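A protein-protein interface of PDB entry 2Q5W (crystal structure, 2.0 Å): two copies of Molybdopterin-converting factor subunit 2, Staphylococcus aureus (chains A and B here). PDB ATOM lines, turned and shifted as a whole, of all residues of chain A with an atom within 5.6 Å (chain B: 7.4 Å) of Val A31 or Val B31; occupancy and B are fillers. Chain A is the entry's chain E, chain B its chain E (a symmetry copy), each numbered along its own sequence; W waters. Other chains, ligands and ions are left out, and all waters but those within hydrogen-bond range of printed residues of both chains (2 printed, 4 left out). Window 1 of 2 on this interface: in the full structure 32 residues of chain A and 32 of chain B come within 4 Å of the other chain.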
ATOM      1  N   ARG A  18      16.305  20.048  12.717  1.00  0.00           N
ATOM      2  CA  ARG A  18      17.284  19.925  11.631  1.00  0.00           C
ATOM      3  C   ARG A  18      17.005  18.659  10.830  1.00  0.00           C
ATOM      4  O   ARG A  18      16.913  18.728   9.615  1.00  0.00           O
ATOM      5  CB  ARG A  18      18.739  19.907  12.127  1.00  0.00           C
ATOM      6  CG  ARG A  18      19.757  19.634  10.999  1.00  0.00           C
ATOM      7  CD  ARG A  18      21.189  19.549  11.508  1.00  0.00           C
ATOM      8  NE  ARG A  18      21.575  20.821  12.133  1.00  0.00           N
ATOM      9  CZ  ARG A  18      21.627  21.070  13.444  1.00  0.00           C
ATOM     10  NH1 ARG A  18      21.330  20.128  14.334  1.00  0.00           N
ATOM     11  NH2 ARG A  18      21.974  22.280  13.868  1.00  0.00           N
ATOM     12  N   VAL A  29      21.812  23.867   6.333  1.00  0.00           N
ATOM     13  CA  VAL A  29      20.740  24.081   7.292  1.00  0.00           C
ATOM     14  C   VAL A  29      21.145  25.222   8.199  1.00  0.00           C
ATOM     15  O   VAL A  29      22.271  25.236   8.722  1.00  0.00           O
ATOM     16  CB  VAL A  29      20.384  22.839   8.127  1.00  0.00           C
ATOM     17  CG1 VAL A  29      19.141  23.117   8.939  1.00  0.00           C
ATOM     18  CG2 VAL A  29      20.122  21.604   7.249  1.00  0.00           C
ATOM     19  N   VAL A  30      20.216  26.161   8.397  1.00  0.00           N
ATOM     20  CA  VAL A  30      20.399  27.209   9.392  1.00  0.00           C
ATOM     21  C   VAL A  30      19.373  27.017  10.491  1.00  0.00           C
ATOM     22  O   VAL A  30      18.171  26.968  10.225  1.00  0.00           O
ATOM     23  CB  VAL A  30      20.298  28.614   8.760  1.00  0.00           C
ATOM     24  CG1 VAL A  30      20.330  29.706   9.831  1.00  0.00           C
ATOM     25  CG2 VAL A  30      21.467  28.783   7.752  1.00  0.00           C
ATOM     26  N   VAL A  31      19.865  26.861  11.710  1.00  0.00           N
ATOM     27  CA  VAL A  31      19.004  26.720  12.891  1.00  0.00           C
ATOM     28  C   VAL A  31      19.237  27.937  13.832  1.00  0.00           C
ATOM     29  O   VAL A  31      20.349  28.154  14.316  1.00  0.00           O
ATOM     30  CB  VAL A  31      19.289  25.416  13.651  1.00  0.00           C
ATOM     31  CG1 VAL A  31      18.464  25.362  14.954  1.00  0.00           C
ATOM     32  CG2 VAL A  31      18.963  24.223  12.791  1.00  0.00           C
ATOM     33  N   PHE A  32      18.175  28.716  14.046  1.00  0.00           N
ATOM     34  CA  PHE A  32      18.167  29.831  14.963  1.00  0.00           C
ATOM     35  C   PHE A  32      17.466  29.377  16.233  1.00  0.00           C
ATOM     36  O   PHE A  32      16.406  28.786  16.147  1.00  0.00           O
ATOM     37  CB  PHE A  32      17.418  31.030  14.352  1.00  0.00           C
ATOM     38  CG  PHE A  32      17.136  32.135  15.350  1.00  0.00           C
ATOM     39  CD1 PHE A  32      18.067  33.113  15.570  1.00  0.00           C
ATOM     40  CD2 PHE A  32      15.939  32.186  16.043  1.00  0.00           C
ATOM     41  CE1 PHE A  32      17.843  34.118  16.515  1.00  0.00           C
ATOM     42  CE2 PHE A  32      15.707  33.200  17.018  1.00  0.00           C
ATOM     43  CZ  PHE A  32      16.683  34.173  17.233  1.00  0.00           C
ATOM     44  N   THR A  33      18.081  29.624  17.377  1.00  0.00           N
ATOM     45  CA  THR A  33      17.437  29.537  18.670  1.00  0.00           C
ATOM     46  C   THR A  33      17.445  30.890  19.407  1.00  0.00           C
ATOM     47  O   THR A  33      18.453  31.619  19.437  1.00  0.00           O
ATOM     48  CB  THR A  33      18.017  28.426  19.535  1.00  0.00           C
ATOM     49  OG1 THR A  33      19.454  28.496  19.561  1.00  0.00           O
ATOM     50  CG2 THR A  33      17.600  27.085  18.992  1.00  0.00           C
ATOM     51  N   LEU A  94      12.732  27.983  18.186  1.00  0.00           N
ATOM     52  CA  LEU A  94      13.698  27.423  17.273  1.00  0.00           C
ATOM     53  C   LEU A  94      13.130  27.410  15.881  1.00  0.00           C
ATOM     54  O   LEU A  94      11.989  26.990  15.670  1.00  0.00           O
ATOM     55  CB  LEU A  94      14.035  25.971  17.652  1.00  0.00           C
ATOM     56  CG  LEU A  94      15.072  25.234  16.773  1.00  0.00           C
ATOM     57  CD1 LEU A  94      15.781  24.193  17.631  1.00  0.00           C
ATOM     58  CD2 LEU A  94      14.451  24.561  15.559  1.00  0.00           C
ATOM     59  N   ILE A  95      13.952  27.847  14.924  1.00  0.00           N
ATOM     60  CA  ILE A  95      13.602  27.845  13.506  1.00  0.00           C
ATOM     61  C   ILE A  95      14.688  27.124  12.737  1.00  0.00           C
ATOM     62  O   ILE A  95      15.846  27.494  12.851  1.00  0.00           O
ATOM     63  CB  ILE A  95      13.558  29.244  12.938  1.00  0.00           C
ATOM     64  CG1 ILE A  95      12.507  30.098  13.655  1.00  0.00           C
ATOM     65  CG2 ILE A  95      13.273  29.225  11.427  1.00  0.00           C
ATOM     66  CD1 ILE A  95      12.745  31.576  13.543  1.00  0.00           C
ATOM     67  N   ALA A  96      14.307  26.127  11.960  1.00  0.00           N
ATOM     68  CA  ALA A  96      15.239  25.388  11.143  1.00  0.00           C
ATOM     69  C   ALA A  96      14.830  25.573   9.699  1.00  0.00           C
ATOM     70  O   ALA A  96      13.688  25.335   9.363  1.00  0.00           O
ATOM     71  CB  ALA A  96      15.200  23.903  11.494  1.00  0.00           C
ATOM     72  N   VAL A  97      15.778  26.020   8.872  1.00  0.00           N
ATOM     73  CA  VAL A  97      15.576  26.110   7.430  1.00  0.00           C
ATOM     74  C   VAL A  97      16.732  25.383   6.701  1.00  0.00           C
ATOM     75  O   VAL A  97      17.917  25.680   6.930  1.00  0.00           O
ATOM     76  CB  VAL A  97      15.473  27.581   6.928  1.00  0.00           C
ATOM     77  CG1 VAL A  97      15.216  27.610   5.465  1.00  0.00           C
ATOM     78  CG2 VAL A  97      14.338  28.305   7.635  1.00  0.00           C
ATOM     79  N   ASN A 109      15.472  32.061   7.206  1.00  0.00           N
ATOM     80  CA  ASN A 109      15.459  31.892   8.647  1.00  0.00           C
ATOM     81  C   ASN A 109      15.234  33.256   9.355  1.00  0.00           C
ATOM     82  O   ASN A 109      14.378  33.382  10.228  1.00  0.00           O
ATOM     83  CB  ASN A 109      16.762  31.206   9.091  1.00  0.00           C
ATOM     84  CG  ASN A 109      16.660  30.642  10.489  1.00  0.00           C
ATOM     85  OD1 ASN A 109      16.519  31.393  11.435  1.00  0.00           O
ATOM     86  ND2 ASN A 109      16.670  29.303  10.616  1.00  0.00           N
ATOM     87  N   THR B  14      25.777  17.856  17.478  1.00  0.00           N
ATOM     88  CA  THR B  14      25.504  19.259  17.291  1.00  0.00           C
ATOM     89  C   THR B  14      25.264  20.119  18.565  1.00  0.00           C
ATOM     90  O   THR B  14      25.743  21.276  18.650  1.00  0.00           O
ATOM     91  CB  THR B  14      24.304  19.407  16.342  1.00  0.00           C
ATOM     92  OG1 THR B  14      23.197  18.647  16.871  1.00  0.00           O
ATOM     93  CG2 THR B  14      24.688  18.875  14.939  1.00  0.00           C
ATOM     94  N   GLU B  15      24.568  19.540  19.531  1.00  0.00           N
ATOM     95  CA  GLU B  15      24.118  20.249  20.721  1.00  0.00           C
ATOM     96  C   GLU B  15      25.264  20.882  21.518  1.00  0.00           C
ATOM     97  O   GLU B  15      25.125  22.004  22.007  1.00  0.00           O
ATOM     98  CB  GLU B  15      23.245  19.319  21.600  1.00  0.00           C
ATOM     99  CG  GLU B  15      21.874  18.959  20.900  1.00  0.00           C
ATOM    100  CD  GLU B  15      21.141  17.703  21.464  1.00  0.00           C
ATOM    101  OE1 GLU B  15      21.630  17.077  22.460  1.00  0.00           O
ATOM    102  OE2 GLU B  15      20.041  17.328  20.908  1.00  0.00           O
ATOM    103  N   TYR B  17      28.021  22.339  20.534  1.00  0.00           N
ATOM    104  CA  TYR B  17      28.528  23.605  19.995  1.00  0.00           C
ATOM    105  C   TYR B  17      27.617  24.804  20.364  1.00  0.00           C
ATOM    106  O   TYR B  17      28.136  25.880  20.747  1.00  0.00           O
ATOM    107  CB  TYR B  17      28.757  23.491  18.482  1.00  0.00           C
ATOM    108  CG  TYR B  17      29.724  22.385  18.211  1.00  0.00           C
ATOM    109  CD1 TYR B  17      29.275  21.092  17.897  1.00  0.00           C
ATOM    110  CD2 TYR B  17      31.088  22.589  18.355  1.00  0.00           C
ATOM    111  CE1 TYR B  17      30.162  20.057  17.684  1.00  0.00           C
ATOM    112  CE2 TYR B  17      32.002  21.543  18.121  1.00  0.00           C
ATOM    113  CZ  TYR B  17      31.532  20.294  17.800  1.00  0.00           C
ATOM    114  OH  TYR B  17      32.427  19.256  17.604  1.00  0.00           O
ATOM    115  N   ARG B  18      26.287  24.624  20.256  1.00  0.00           N
ATOM    116  CA  ARG B  18      25.339  25.618  20.773  1.00  0.00           C
ATOM    117  C   ARG B  18      25.581  25.832  22.261  1.00  0.00           C
ATOM    118  O   ARG B  18      25.716  26.967  22.688  1.00  0.00           O
ATOM    119  CB  ARG B  18      23.870  25.230  20.542  1.00  0.00           C
ATOM    120  CG  ARG B  18      22.877  26.204  21.212  1.00  0.00           C
ATOM    121  CD  ARG B  18      21.427  25.776  21.038  1.00  0.00           C
ATOM    122  NE  ARG B  18      21.084  25.731  19.610  1.00  0.00           N
ATOM    123  CZ  ARG B  18      21.002  24.632  18.855  1.00  0.00           C
ATOM    124  NH1 ARG B  18      21.223  23.427  19.370  1.00  0.00           N
ATOM    125  NH2 ARG B  18      20.703  24.745  17.566  1.00  0.00           N
ATOM    126  N   GLU B  19      25.696  24.753  23.030  1.00  0.00           N
ATOM    127  CA  GLU B  19      25.873  24.856  24.456  1.00  0.00           C
ATOM    128  C   GLU B  19      27.168  25.617  24.813  1.00  0.00           C
ATOM    129  O   GLU B  19      27.181  26.399  25.741  1.00  0.00           O
ATOM    130  CB  GLU B  19      25.910  23.474  25.118  1.00  0.00           C
ATOM    131  CG  GLU B  19      24.651  22.640  24.874  1.00  0.00           C
ATOM    132  CD  GLU B  19      24.687  21.245  25.519  1.00  0.00           C
ATOM    133  OE1 GLU B  19      25.774  20.580  25.472  1.00  0.00           O
ATOM    134  OE2 GLU B  19      23.614  20.808  26.032  1.00  0.00           O
ATOM    135  N   THR B  21      28.507  28.068  23.201  1.00  0.00           N
ATOM    136  CA  THR B  21      28.306  29.478  22.901  1.00  0.00           C
ATOM    137  C   THR B  21      27.272  30.191  23.787  1.00  0.00           C
ATOM    138  O   THR B  21      27.242  31.408  23.823  1.00  0.00           O
ATOM    139  CB  THR B  21      27.921  29.719  21.436  1.00  0.00           C
ATOM    140  OG1 THR B  21      26.583  29.268  21.219  1.00  0.00           O
ATOM    141  CG2 THR B  21      28.927  29.024  20.485  1.00  0.00           C
ATOM    142  N   VAL B  29      21.190  32.268  19.139  1.00  0.00           N
ATOM    143  CA  VAL B  29      22.240  31.422  18.595  1.00  0.00           C
ATOM    144  C   VAL B  29      21.863  31.068  17.173  1.00  0.00           C
ATOM    145  O   VAL B  29      20.723  30.650  16.913  1.00  0.00           O
ATOM    146  CB  VAL B  29      22.506  30.145  19.408  1.00  0.00           C
ATOM    147  CG1 VAL B  29      23.733  29.449  18.869  1.00  0.00           C
ATOM    148  CG2 VAL B  29      22.734  30.442  20.900  1.00  0.00           C
ATOM    149  N   VAL B  30      22.831  31.214  16.264  1.00  0.00           N
ATOM    150  CA  VAL B  30      22.668  30.731  14.899  1.00  0.00           C
ATOM    151  C   VAL B  30      23.647  29.597  14.669  1.00  0.00           C
ATOM    152  O   VAL B  30      24.852  29.761  14.859  1.00  0.00           O
ATOM    153  CB  VAL B  30      22.860  31.866  13.870  1.00  0.00           C
ATOM    154  CG1 VAL B  30      22.848  31.323  12.441  1.00  0.00           C
ATOM    155  CG2 VAL B  30      21.735  32.915  14.082  1.00  0.00           C
ATOM    156  N   VAL B  31      23.107  28.443  14.306  1.00  0.00           N
ATOM    157  CA  VAL B  31      23.921  27.263  13.990  1.00  0.00           C
ATOM    158  C   VAL B  31      23.719  26.899  12.491  1.00  0.00           C
ATOM    159  O   VAL B  31      22.604  26.598  12.062  1.00  0.00           O
ATOM    160  CB  VAL B  31      23.547  26.061  14.869  1.00  0.00           C
ATOM    161  CG1 VAL B  31      24.325  24.805  14.424  1.00  0.00           C
ATOM    162  CG2 VAL B  31      23.841  26.355  16.317  1.00  0.00           C
ATOM    163  N   PHE B  32      24.811  26.961  11.727  1.00  0.00           N
ATOM    164  CA  PHE B  32      24.845  26.566  10.339  1.00  0.00           C
ATOM    165  C   PHE B  32      25.481  25.188  10.267  1.00  0.00           C
ATOM    166  O   PHE B  32      26.512  24.977  10.878  1.00  0.00           O
ATOM    167  CB  PHE B  32      25.673  27.567   9.510  1.00  0.00           C
ATOM    168  CG  PHE B  32      25.977  27.080   8.108  1.00  0.00           C
ATOM    169  CD1 PHE B  32      25.089  27.316   7.094  1.00  0.00           C
ATOM    170  CD2 PHE B  32      27.151  26.406   7.823  1.00  0.00           C
ATOM    171  CE1 PHE B  32      25.332  26.841   5.803  1.00  0.00           C
ATOM    172  CE2 PHE B  32      27.402  25.907   6.510  1.00  0.00           C
ATOM    173  CZ  PHE B  32      26.469  26.147   5.502  1.00  0.00           C
ATOM    174  N   THR B  33      24.841  24.270   9.563  1.00  0.00           N
ATOM    175  CA  THR B  33      25.437  23.019   9.145  1.00  0.00           C
ATOM    176  C   THR B  33      25.473  22.885   7.610  1.00  0.00           C
ATOM    177  O   THR B  33      24.502  23.199   6.898  1.00  0.00           O
ATOM    178  CB  THR B  33      24.775  21.813   9.796  1.00  0.00           C
ATOM    179  OG1 THR B  33      23.342  21.888   9.674  1.00  0.00           O
ATOM    180  CG2 THR B  33      25.141  21.753  11.255  1.00  0.00           C
ATOM    181  N   VAL B  93      30.431  20.363   8.179  1.00  0.00           N
ATOM    182  CA  VAL B  93      30.873  21.540   8.898  1.00  0.00           C
ATOM    183  C   VAL B  93      29.729  22.083   9.759  1.00  0.00           C
ATOM    184  O   VAL B  93      28.569  22.053   9.357  1.00  0.00           O
ATOM    185  CB  VAL B  93      31.423  22.658   7.910  1.00  0.00           C
ATOM    186  CG1 VAL B  93      30.335  23.183   6.926  1.00  0.00           C
ATOM    187  CG2 VAL B  93      32.024  23.812   8.670  1.00  0.00           C
ATOM    188  N   LEU B  94      30.072  22.606  10.916  1.00  0.00           N
ATOM    189  CA  LEU B  94      29.110  23.266  11.763  1.00  0.00           C
ATOM    190  C   LEU B  94      29.721  24.507  12.352  1.00  0.00           C
ATOM    191  O   LEU B  94      30.846  24.475  12.858  1.00  0.00           O
ATOM    192  CB  LEU B  94      28.688  22.357  12.929  1.00  0.00           C
ATOM    193  CG  LEU B  94      27.645  22.919  13.923  1.00  0.00           C
ATOM    194  CD1 LEU B  94      26.857  21.753  14.508  1.00  0.00           C
ATOM    195  CD2 LEU B  94      28.271  23.731  15.046  1.00  0.00           C
ATOM    196  N   ILE B  95      28.955  25.599  12.308  1.00  0.00           N
ATOM    197  CA  ILE B  95      29.350  26.879  12.890  1.00  0.00           C
ATOM    198  C   ILE B  95      28.255  27.349  13.824  1.00  0.00           C
ATOM    199  O   ILE B  95      27.113  27.450  13.401  1.00  0.00           O
ATOM    200  CB  ILE B  95      29.483  27.955  11.839  1.00  0.00           C
ATOM    201  CG1 ILE B  95      30.551  27.587  10.805  1.00  0.00           C
ATOM    202  CG2 ILE B  95      29.815  29.317  12.472  1.00  0.00           C
ATOM    203  CD1 ILE B  95      30.391  28.292   9.488  1.00  0.00           C
ATOM    204  N   ALA B  96      28.611  27.644  15.060  1.00  0.00           N
ATOM    205  CA  ALA B  96      27.670  28.143  16.034  1.00  0.00           C
ATOM    206  C   ALA B  96      28.135  29.519  16.457  1.00  0.00           C
ATOM    207  O   ALA B  96      29.274  29.674  16.847  1.00  0.00           O
ATOM    208  CB  ALA B  96      27.623  27.227  17.254  1.00  0.00           C
ATOM    209  N   VAL B  97      27.238  30.502  16.348  1.00  0.00           N
ATOM    210  CA  VAL B  97      27.492  31.847  16.851  1.00  0.00           C
ATOM    211  C   VAL B  97      26.325  32.283  17.770  1.00  0.00           C
ATOM    212  O   VAL B  97      25.149  32.251  17.369  1.00  0.00           O
ATOM    213  CB  VAL B  97      27.685  32.889  15.709  1.00  0.00           C
ATOM    214  CG1 VAL B  97      27.991  34.227  16.278  1.00  0.00           C
ATOM    215  CG2 VAL B  97      28.830  32.474  14.799  1.00  0.00           C
ATOM    216  N   SER B  98      26.696  32.718  18.970  1.00  0.00           N
ATOM    217  CA  SER B  98      25.782  33.346  19.916  1.00  0.00           C
ATOM    218  C   SER B  98      25.984  34.839  19.963  1.00  0.00           C
ATOM    219  O   SER B  98      27.067  35.346  19.615  1.00  0.00           O
ATOM    220  CB  SER B  98      25.963  32.750  21.319  1.00  0.00           C
ATOM    221  OG  SER B  98      27.209  33.104  21.916  1.00  0.00           O
ATOM    222  N   ALA B 105      24.503  37.577  15.135  1.00  0.00           N
ATOM    223  CA  ALA B 105      24.665  36.119  15.097  1.00  0.00           C
ATOM    224  C   ALA B 105      24.498  35.609  13.658  1.00  0.00           C
ATOM    225  O   ALA B 105      25.278  34.791  13.208  1.00  0.00           O
ATOM    226  CB  ALA B 105      23.682  35.409  16.045  1.00  0.00           C
ATOM    227  N   TYR B 106      23.533  36.143  12.922  1.00  0.00           N
ATOM    228  CA  TYR B 106      23.388  35.740  11.530  1.00  0.00           C
ATOM    229  C   TYR B 106      24.580  36.193  10.667  1.00  0.00           C
ATOM    230  O   TYR B 106      25.150  35.388   9.879  1.00  0.00           O
ATOM    231  CB  TYR B 106      22.104  36.278  10.955  1.00  0.00           C
ATOM    232  CG  TYR B 106      20.802  35.571  11.340  1.00  0.00           C
ATOM    233  CD1 TYR B 106      19.894  36.188  12.172  1.00  0.00           C
ATOM    234  CD2 TYR B 106      20.451  34.328  10.838  1.00  0.00           C
ATOM    235  CE1 TYR B 106      18.693  35.609  12.490  1.00  0.00           C
ATOM    236  CE2 TYR B 106      19.227  33.747  11.170  1.00  0.00           C
ATOM    237  CZ  TYR B 106      18.362  34.388  12.009  1.00  0.00           C
ATOM    238  OH  TYR B 106      17.103  33.875  12.329  1.00  0.00           O
ATOM    239  N   ASN B 109      27.900  34.423  11.496  1.00  0.00           N
ATOM    240  CA  ASN B 109      27.858  33.036  11.073  1.00  0.00           C
ATOM    241  C   ASN B 109      28.128  32.921   9.548  1.00  0.00           C
ATOM    242  O   ASN B 109      28.960  32.129   9.111  1.00  0.00           O
ATOM    243  CB  ASN B 109      26.508  32.421  11.481  1.00  0.00           C
ATOM    244  CG  ASN B 109      26.536  30.911  11.440  1.00  0.00           C
ATOM    245  OD1 ASN B 109      26.684  30.337  10.377  1.00  0.00           O
ATOM    246  ND2 ASN B 109      26.455  30.260  12.614  1.00  0.00           N
HETATM  247  O   HOH W   1      22.190  23.766  11.398  1.00  0.00           O
HETATM  248  O   HOH W   2      20.642  27.610  17.189  1.00  0.00           O
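The guanidinium group (NH1) of Arg A18 is in hydrogen-bond range of the side-chain hydroxyl (OG1) of Thr B14, at 3.5 Å.
The guanidinium group (NE) of Arg A18 sits at hydrogen-bond distance from the side-chain hydroxyl (OG1) of Thr B33, 3.2 Å away.
The backbone NH of Val A29 lies within hydrogen-bond range of the backbone carbonyl oxygen of Thr B33, 2.8 Å away.
N of Val A31 sits at hydrogen-bond distance from O of Val B31 (2.8 Å).
The side-chain hydroxyl of Thr A33 lies within hydrogen-bond range of the guanidinium group of Arg B18, 3.2 Å away.
The backbone carbonyl oxygen (O) of Thr A33 is in hydrogen-bond range of the backbone NH (N) of Val B29 (2.8 Å).
OH of Tyr B106 lies within hydrogen-bond range of OD1 of Asn A109 (2.7 Å).
The backbone carbonyl oxygen (O) of Val A30 is in hydrogen-bond range of the side-chain amide nitrogen (ND2) of Asn A109 (2.8 Å).
The backbone NH (N) of Phe A32 sits at hydrogen-bond distance from the backbone carbonyl oxygen (O) of Ile A95, 2.9 Å away.
The backbone carbonyl oxygen (O) of Ile A95 is in hydrogen-bond range of the side-chain amide nitrogen (ND2) of Asn A109 (3.0 Å).
The backbone NH of Val B30 is in hydrogen-bond range of the backbone carbonyl oxygen of Val B97 (2.8 Å).
The side-chain amide nitrogen of Asn B109 is in hydrogen-bond range of the backbone carbonyl oxygen of Val B30, at 2.8 Å.
O of Ile B95 is in hydrogen-bond range of N of Phe B32, 2.9 Å away.
Among the printed residues, merely in contact across the chains: Phe A32 with Val B29 (3.3 Å), Val A29 with Phe B32 (3.3 Å), Phe A32 with Tyr B106 (3.5 Å), Arg A18 with Val B31 (3.5 Å), Val A31 with Arg B18 (3.5 Å), Val A31 with Val B30 (3.5 Å), Val A30 with Val B31 (3.5 Å), Val A31 with Val B29 (3.6 Å), Val A29 with Val B31 (3.6 Å), Val A30 with Phe B32 (3.96 Å), Phe A32 with Val B30 (3.96 Å) and Val A30 with Val B30 (3.97 Å).
Printed residues of chain B within 4 Å of Val A29: Val B31, Phe B32 and Thr B33.
Of the printed residues of chain B, Thr A33 touches Arg B18 (3.2 Å) and Val B29 (2.8 Å).
Leu A94 touches none of the printed residues of chain B.
Of the printed residues of chain B, Asn A109 touches Tyr B106.
Printed residues of chain A within 4 Å of Thr B14: Arg A18 (3.5 Å).
Of the printed residues of chain A, Val B30 touches Val A30, Val A31 and Phe A32.
The nearest residue of chain B that does not touch Val A31 is Phe B32 (4.9 Å).
The nearest printed residue of chain B that does not touch Arg A18 is Arg B18 (4.6 Å).
Of the 11 printed residues of chain A, 7 touch a printed residue of chain B.
Hydrophobic or aromatic side chains of chain A that line the printed part of chain B: Val A29, Val A30, Val A31 and Phe A32.
Hydrophobic or aromatic side chains of chain B within 4 Å of the printed part of chain A: Val B29, Val B30, Val B31, Phe B32 and Tyr B106.
Among the printed residues, no Asp or Glu carboxylate lies within 4 Å of a Lys or Arg side-chain nitrogen of the other chain.
Val A29 touches Val B31, and with the chains exchanged Val A31 touches Val B29.
Val B30 touches its own counterpart, Val A30.
Val A30 touches Phe B32, and with the chains exchanged Phe A32 touches Val B30.
Val B31 touches its own counterpart, Val A31.
Of the 19 pairs that touch across the chains among the printed residues, 16 have their exchanged pair printed and touching as well.
Water W2 lies within hydrogen-bond range of the side-chain hydroxyl (OG1) of Thr A33 (2.8 Å), the guanidinium group (NH2) of Arg B18 (2.9 Å), the backbone carbonyl oxygen (O) of Val A31 (2.9 Å) and the backbone carbonyl oxygen (O) of Val B29 (3.1 Å).
Water W1 lies within hydrogen-bond range of the side-chain hydroxyl of Thr B33 (2.8 Å), the guanidinium group of Arg A18 (2.9 Å), the backbone carbonyl oxygen of Val B31 (2.9 Å) and the backbone carbonyl oxygen of Val A29 (3.1 Å).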
